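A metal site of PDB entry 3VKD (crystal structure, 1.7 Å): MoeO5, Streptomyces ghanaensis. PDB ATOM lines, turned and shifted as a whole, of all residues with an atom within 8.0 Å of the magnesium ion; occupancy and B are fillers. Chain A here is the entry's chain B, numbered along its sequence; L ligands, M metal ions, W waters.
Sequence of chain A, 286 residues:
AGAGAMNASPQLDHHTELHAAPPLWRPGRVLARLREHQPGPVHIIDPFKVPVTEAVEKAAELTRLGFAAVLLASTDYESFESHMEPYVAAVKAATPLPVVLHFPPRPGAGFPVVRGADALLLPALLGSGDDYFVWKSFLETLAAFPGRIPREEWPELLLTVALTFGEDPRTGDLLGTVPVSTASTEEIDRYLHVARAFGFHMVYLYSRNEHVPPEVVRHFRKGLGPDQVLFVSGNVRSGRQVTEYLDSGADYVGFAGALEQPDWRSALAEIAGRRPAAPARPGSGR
The side-chain carboxylate (OD1) of Asp 46 sits at hydrogen-bond distance from the backbone NH (N) of Lys 49 (3.4 Å).
OD1 of Asp 46 sits at hydrogen-bond distance from N of Phe 48.
The side-chain hydroxyl of Thr 75 lies within hydrogen-bond range of the guanidinium group of Arg 208.
Merely in contact with the magnesium ion: Thr 75.
Four residues have an atom within 4 Å of the magnesium ion: Asp 46, Ser 74, Thr 75 and Asp 76.
The nearest printed residue that does not touch the magnesium ion is Lys 49 (4.6 Å).
The magnesium ion is bound by water W2, the side-chain hydroxyl (OG) of Ser 74, the side-chain carboxylate (OD1) of Asp 76, water W1 and the side-chain carboxylate (OD2) of Asp 46.
The magnesium ion has five donor atoms within binding distance.
Slightly farther from the magnesium ion lies an oxygen (O2) of LIG L1 (2.7 Å).
Slightly farther from the magnesium ion lies an oxygen (O3) of LIG L1 (2.8 Å).
Water W2 bridges the side-chain carboxylate of Asp 76 (2.4 Å) and the side-chain carboxylate of Asp 46 (2.9 Å).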
ATOM      1  N   ILE A  45      -3.296  -9.042  28.915  1.00  0.00           N
ATOM      2  CA  ILE A  45      -3.538  -8.388  30.198  1.00  0.00           C
ATOM      3  C   ILE A  45      -4.483  -7.208  29.917  1.00  0.00           C
ATOM      4  O   ILE A  45      -4.177  -6.389  29.074  1.00  0.00           O
ATOM      5  CB  ILE A  45      -2.238  -7.836  30.773  1.00  0.00           C
ATOM      6  CG1 ILE A  45      -1.305  -8.988  31.159  1.00  0.00           C
ATOM      7  CG2 ILE A  45      -2.579  -6.952  32.018  1.00  0.00           C
ATOM      8  CD1 ILE A  45       0.156  -8.504  31.458  1.00  0.00           C
ATOM      9  N   ASP A  46      -5.610  -7.145  30.623  1.00  0.00           N
ATOM     10  CA  ASP A  46      -6.554  -6.007  30.469  1.00  0.00           C
ATOM     11  C   ASP A  46      -6.019  -4.980  31.495  1.00  0.00           C
ATOM     12  O   ASP A  46      -6.258  -5.146  32.684  1.00  0.00           O
ATOM     13  CB  ASP A  46      -7.934  -6.477  30.881  1.00  0.00           C
ATOM     14  CG  ASP A  46      -8.951  -5.393  30.753  1.00  0.00           C
ATOM     15  OD1 ASP A  46      -8.588  -4.258  30.959  1.00  0.00           O
ATOM     16  OD2 ASP A  46     -10.119  -5.690  30.437  1.00  0.00           O
ATOM     17  N   PRO A  47      -5.338  -3.923  31.048  1.00  0.00           N
ATOM     18  CA  PRO A  47      -4.735  -2.937  31.954  1.00  0.00           C
ATOM     19  C   PRO A  47      -5.667  -2.056  32.728  1.00  0.00           C
ATOM     20  O   PRO A  47      -5.261  -1.412  33.707  1.00  0.00           O
ATOM     21  CB  PRO A  47      -3.745  -2.175  31.080  1.00  0.00           C
ATOM     22  CG  PRO A  47      -4.269  -2.304  29.690  1.00  0.00           C
ATOM     23  CD  PRO A  47      -5.265  -3.461  29.631  1.00  0.00           C
ATOM     24  N   PHE A  48      -6.919  -2.081  32.379  1.00  0.00           N
ATOM     25  CA  PHE A  48      -7.894  -1.242  33.122  1.00  0.00           C
ATOM     26  C   PHE A  48      -8.636  -2.070  34.152  1.00  0.00           C
ATOM     27  O   PHE A  48      -9.596  -1.591  34.851  1.00  0.00           O
ATOM     28  CB  PHE A  48      -8.818  -0.553  32.111  1.00  0.00           C
ATOM     29  CG  PHE A  48      -8.089   0.492  31.282  1.00  0.00           C
ATOM     30  CD1 PHE A  48      -7.513   0.183  30.019  1.00  0.00           C
ATOM     31  CD2 PHE A  48      -7.837   1.759  31.830  1.00  0.00           C
ATOM     32  CE1 PHE A  48      -6.709   1.111  29.377  1.00  0.00           C
ATOM     33  CE2 PHE A  48      -7.054   2.681  31.191  1.00  0.00           C
ATOM     34  CZ  PHE A  48      -6.466   2.360  29.944  1.00  0.00           C
ATOM     35  N   LYS A  49      -8.274  -3.342  34.236  1.00  0.00           N
ATOM     36  CA  LYS A  49      -8.874  -4.244  35.246  1.00  0.00           C
ATOM     37  C   LYS A  49      -7.777  -4.869  36.104  1.00  0.00           C
ATOM     38  O   LYS A  49      -8.009  -5.173  37.291  1.00  0.00           O
ATOM     39  CB  LYS A  49      -9.694  -5.376  34.581  1.00  0.00           C
ATOM     40  CG  LYS A  49     -10.260  -6.342  35.548  1.00  0.00           C
ATOM     41  CD  LYS A  49     -10.845  -7.629  34.885  1.00  0.00           C
ATOM     42  CE  LYS A  49     -11.555  -7.307  33.559  1.00  0.00           C
ATOM     43  NZ  LYS A  49     -12.706  -6.397  33.718  1.00  0.00           N
ATOM     44  N   VAL A  50      -6.592  -5.062  35.544  1.00  0.00           N
ATOM     45  CA  VAL A  50      -5.498  -5.743  36.263  1.00  0.00           C
ATOM     46  C   VAL A  50      -4.579  -4.700  36.852  1.00  0.00           C
ATOM     47  O   VAL A  50      -4.061  -3.852  36.165  1.00  0.00           O
ATOM     48  CB  VAL A  50      -4.698  -6.621  35.300  1.00  0.00           C
ATOM     49  CG1 VAL A  50      -3.538  -7.242  35.996  1.00  0.00           C
ATOM     50  CG2 VAL A  50      -5.664  -7.731  34.727  1.00  0.00           C
ATOM     51  N   ALA A  73      -4.857  -5.174  26.387  1.00  0.00           N
ATOM     52  CA  ALA A  73      -6.062  -4.923  25.606  1.00  0.00           C
ATOM     53  C   ALA A  73      -7.306  -4.810  26.436  1.00  0.00           C
ATOM     54  O   ALA A  73      -7.453  -5.518  27.436  1.00  0.00           O
ATOM     55  CB  ALA A  73      -6.271  -6.114  24.570  1.00  0.00           C
ATOM     56  N   SER A  74      -8.235  -3.964  25.990  1.00  0.00           N
ATOM     57  CA  SER A  74      -9.494  -3.865  26.693  1.00  0.00           C
ATOM     58  C   SER A  74     -10.494  -3.212  25.756  1.00  0.00           C
ATOM     59  O   SER A  74     -10.117  -2.452  24.871  1.00  0.00           O
ATOM     60  CB  SER A  74      -9.306  -2.951  27.934  1.00  0.00           C
ATOM     61  OG  SER A  74     -10.530  -2.889  28.631  1.00  0.00           O
ATOM     62  N   THR A  75     -11.771  -3.476  25.969  1.00  0.00           N
ATOM     63  CA  THR A  75     -12.819  -2.843  25.165  1.00  0.00           C
ATOM     64  C   THR A  75     -13.016  -1.444  25.724  1.00  0.00           C
ATOM     65  O   THR A  75     -13.231  -0.475  24.988  1.00  0.00           O
ATOM     66  CB  THR A  75     -14.129  -3.617  25.332  1.00  0.00           C
ATOM     67  OG1 THR A  75     -13.968  -4.909  24.689  1.00  0.00           O
ATOM     68  CG2 THR A  75     -15.331  -2.881  24.683  1.00  0.00           C
ATOM     69  N   ASP A  76     -12.948  -1.350  27.058  1.00  0.00           N
ATOM     70  CA  ASP A  76     -13.135  -0.073  27.776  1.00  0.00           C
ATOM     71  C   ASP A  76     -11.817   0.572  28.189  1.00  0.00           C
ATOM     72  O   ASP A  76     -10.879  -0.112  28.491  1.00  0.00           O
ATOM     73  CB  ASP A  76     -13.868  -0.332  29.115  1.00  0.00           C
ATOM     74  CG  ASP A  76     -13.201  -1.434  29.913  1.00  0.00           C
ATOM     75  OD1 ASP A  76     -13.266  -2.606  29.457  1.00  0.00           O
ATOM     76  OD2 ASP A  76     -12.582  -1.151  30.978  1.00  0.00           O
ATOM     77  N   TYR A  77     -11.753   1.897  28.216  1.00  0.00           N
ATOM     78  CA  TYR A  77     -10.576   2.574  28.712  1.00  0.00           C
ATOM     79  C   TYR A  77     -10.932   4.046  29.000  1.00  0.00           C
ATOM     80  O   TYR A  77     -11.868   4.595  28.391  1.00  0.00           O
ATOM     81  CB  TYR A  77      -9.392   2.490  27.724  1.00  0.00           C
ATOM     82  CG  TYR A  77      -9.685   3.029  26.359  1.00  0.00           C
ATOM     83  CD1 TYR A  77     -10.120   2.184  25.340  1.00  0.00           C
ATOM     84  CD2 TYR A  77      -9.441   4.393  26.046  1.00  0.00           C
ATOM     85  CE1 TYR A  77     -10.296   2.660  24.038  1.00  0.00           C
ATOM     86  CE2 TYR A  77      -9.599   4.864  24.727  1.00  0.00           C
ATOM     87  CZ  TYR A  77     -10.026   3.983  23.741  1.00  0.00           C
ATOM     88  OH  TYR A  77     -10.149   4.391  22.411  1.00  0.00           O
ATOM     89  N   PHE A 103      -6.885  -1.835  21.425  1.00  0.00           N
ATOM     90  CA  PHE A 103      -8.047  -1.109  21.956  1.00  0.00           C
ATOM     91  C   PHE A 103      -8.871  -0.553  20.806  1.00  0.00           C
ATOM     92  O   PHE A 103      -8.324  -0.299  19.722  1.00  0.00           O
ATOM     93  CB  PHE A 103      -7.572   0.107  22.765  1.00  0.00           C
ATOM     94  CG  PHE A 103      -6.741  -0.269  23.955  1.00  0.00           C
ATOM     95  CD1 PHE A 103      -7.376  -0.574  25.185  1.00  0.00           C
ATOM     96  CD2 PHE A 103      -5.370  -0.417  23.845  1.00  0.00           C
ATOM     97  CE1 PHE A 103      -6.612  -1.011  26.271  1.00  0.00           C
ATOM     98  CE2 PHE A 103      -4.590  -0.856  24.906  1.00  0.00           C
ATOM     99  CZ  PHE A 103      -5.202  -1.142  26.114  1.00  0.00           C
ATOM    100  N   ARG A 170     -22.634  -6.026  23.325  1.00  0.00           N
ATOM    101  CA  ARG A 170     -21.705  -5.052  23.864  1.00  0.00           C
ATOM    102  C   ARG A 170     -20.813  -4.493  22.715  1.00  0.00           C
ATOM    103  O   ARG A 170     -20.707  -3.259  22.521  1.00  0.00           O
ATOM    104  CB  ARG A 170     -20.767  -5.669  24.910  1.00  0.00           C
ATOM    105  CG  ARG A 170     -19.772  -4.632  25.480  1.00  0.00           C
ATOM    106  CD  ARG A 170     -18.972  -5.162  26.683  1.00  0.00           C
ATOM    107  NE  ARG A 170     -19.769  -5.315  27.882  1.00  0.00           N
ATOM    108  CZ  ARG A 170     -20.097  -4.322  28.727  1.00  0.00           C
ATOM    109  NH1 ARG A 170     -19.692  -3.079  28.506  1.00  0.00           N
ATOM    110  NH2 ARG A 170     -20.844  -4.585  29.794  1.00  0.00           N
ATOM    111  N   ARG A 208     -16.835 -12.722  22.067  1.00  0.00           N
ATOM    112  CA  ARG A 208     -16.950 -12.297  23.446  1.00  0.00           C
ATOM    113  C   ARG A 208     -17.671 -13.335  24.307  1.00  0.00           C
ATOM    114  O   ARG A 208     -17.250 -13.621  25.426  1.00  0.00           O
ATOM    115  CB  ARG A 208     -17.777 -10.989  23.546  1.00  0.00           C
ATOM    116  CG  ARG A 208     -17.740 -10.390  24.993  1.00  0.00           C
ATOM    117  CD  ARG A 208     -18.549  -9.058  25.082  1.00  0.00           C
ATOM    118  NE  ARG A 208     -17.894  -8.037  24.245  1.00  0.00           N
ATOM    119  CZ  ARG A 208     -16.836  -7.326  24.608  1.00  0.00           C
ATOM    120  NH1 ARG A 208     -16.236  -7.508  25.813  1.00  0.00           N
ATOM    121  NH2 ARG A 208     -16.340  -6.429  23.769  1.00  0.00           N
ATOM    122  N   GLU A 260      -7.708 -13.717  35.396  1.00  0.00           N
ATOM    123  CA  GLU A 260      -8.224 -12.602  36.219  1.00  0.00           C
ATOM    124  C   GLU A 260      -8.849 -13.175  37.480  1.00  0.00           C
ATOM    125  O   GLU A 260     -10.065 -13.070  37.722  1.00  0.00           O
ATOM    126  CB  GLU A 260      -9.243 -11.799  35.394  1.00  0.00           C
ATOM    127  CG  GLU A 260      -8.502 -11.144  34.230  1.00  0.00           C
ATOM    128  CD  GLU A 260      -9.433 -10.477  33.216  1.00  0.00           C
ATOM    129  OE1 GLU A 260     -10.667 -10.483  33.436  1.00  0.00           O
ATOM    130  OE2 GLU A 260      -8.932  -9.932  32.199  1.00  0.00           O
HETATM  131  P1  LIG L   1     -13.194  -6.201  27.736  1.00  0.00           P
HETATM  132  O1  LIG L   1     -13.761  -6.370  26.410  1.00  0.00           O
HETATM  133  O2  LIG L   1     -11.821  -5.577  27.646  1.00  0.00           O
HETATM  134  O3  LIG L   1     -14.038  -5.251  28.642  1.00  0.00           O
HETATM  135  O4  LIG L   1     -13.165  -7.709  28.488  1.00  0.00           O
HETATM  136  P1  LG2 L   2     -11.142 -13.528  27.135  1.00  0.00           P
HETATM  137  C1  LG2 L   2     -11.408  -8.318  24.892  1.00  0.00           C
HETATM  138  C2  LG2 L   2     -11.498  -8.363  23.375  1.00  0.00           C
HETATM  139  C3  LG2 L   2     -10.711  -7.694  22.529  1.00  0.00           C
HETATM  140  C4  LG2 L   2     -11.002  -7.975  21.069  1.00  0.00           C
HETATM  141  C5  LG2 L   2      -9.567  -6.741  22.928  1.00  0.00           C
HETATM  142  C6  LG2 L   2     -10.133  -5.301  22.879  1.00  0.00           C
HETATM  143  C7  LG2 L   2     -10.099  -4.669  21.489  1.00  0.00           C
HETATM  144  C8  LG2 L   2     -11.218  -4.220  20.838  1.00  0.00           C
HETATM  145  C9  LG2 L   2     -12.654  -4.272  21.370  1.00  0.00           C
HETATM  146  C10 LG2 L   2      -9.913 -11.846  25.564  1.00  0.00           C
HETATM  147  O1  LG2 L   2     -11.170 -12.516  25.837  1.00  0.00           O
HETATM  148  C11 LG2 L   2     -10.335 -10.669  24.640  1.00  0.00           C
HETATM  149  O2  LG2 L   2     -10.866  -9.711  25.452  1.00  0.00           O
HETATM  150  C12 LG2 L   2      -9.065 -10.235  23.888  1.00  0.00           C
HETATM  151  C13 LG2 L   2     -10.976  -3.614  19.466  1.00  0.00           C
HETATM  152  C14 LG2 L   2     -11.848  -4.184  18.300  1.00  0.00           C
HETATM  153  C15 LG2 L   2     -11.449  -5.601  17.983  1.00  0.00           C
HETATM  154  C16 LG2 L   2     -12.253  -6.681  18.000  1.00  0.00           C
HETATM  155  C17 LG2 L   2     -13.742  -6.596  18.345  1.00  0.00           C
HETATM  156  C18 LG2 L   2     -11.618  -7.997  17.639  1.00  0.00           C
HETATM  157  O3  LG2 L   2      -9.917 -14.455  27.103  1.00  0.00           O
HETATM  158  O4  LG2 L   2      -8.846 -10.805  22.819  1.00  0.00           O
HETATM  159  O5  LG2 L   2     -11.226 -12.664  28.419  1.00  0.00           O
HETATM  160  O6  LG2 L   2      -8.330  -9.306  24.338  1.00  0.00           O
HETATM  161  O7  LG2 L   2     -12.448 -14.268  26.951  1.00  0.00           O
HETATM  162 MG    MG M   1     -11.776  -4.099  29.873  1.00  0.00          MG
HETATM  163  O   HOH W   1     -13.036  -5.800  30.911  1.00  0.00           O
HETATM  164  O   HOH W   2     -11.195  -3.080  31.518  1.00  0.00           O
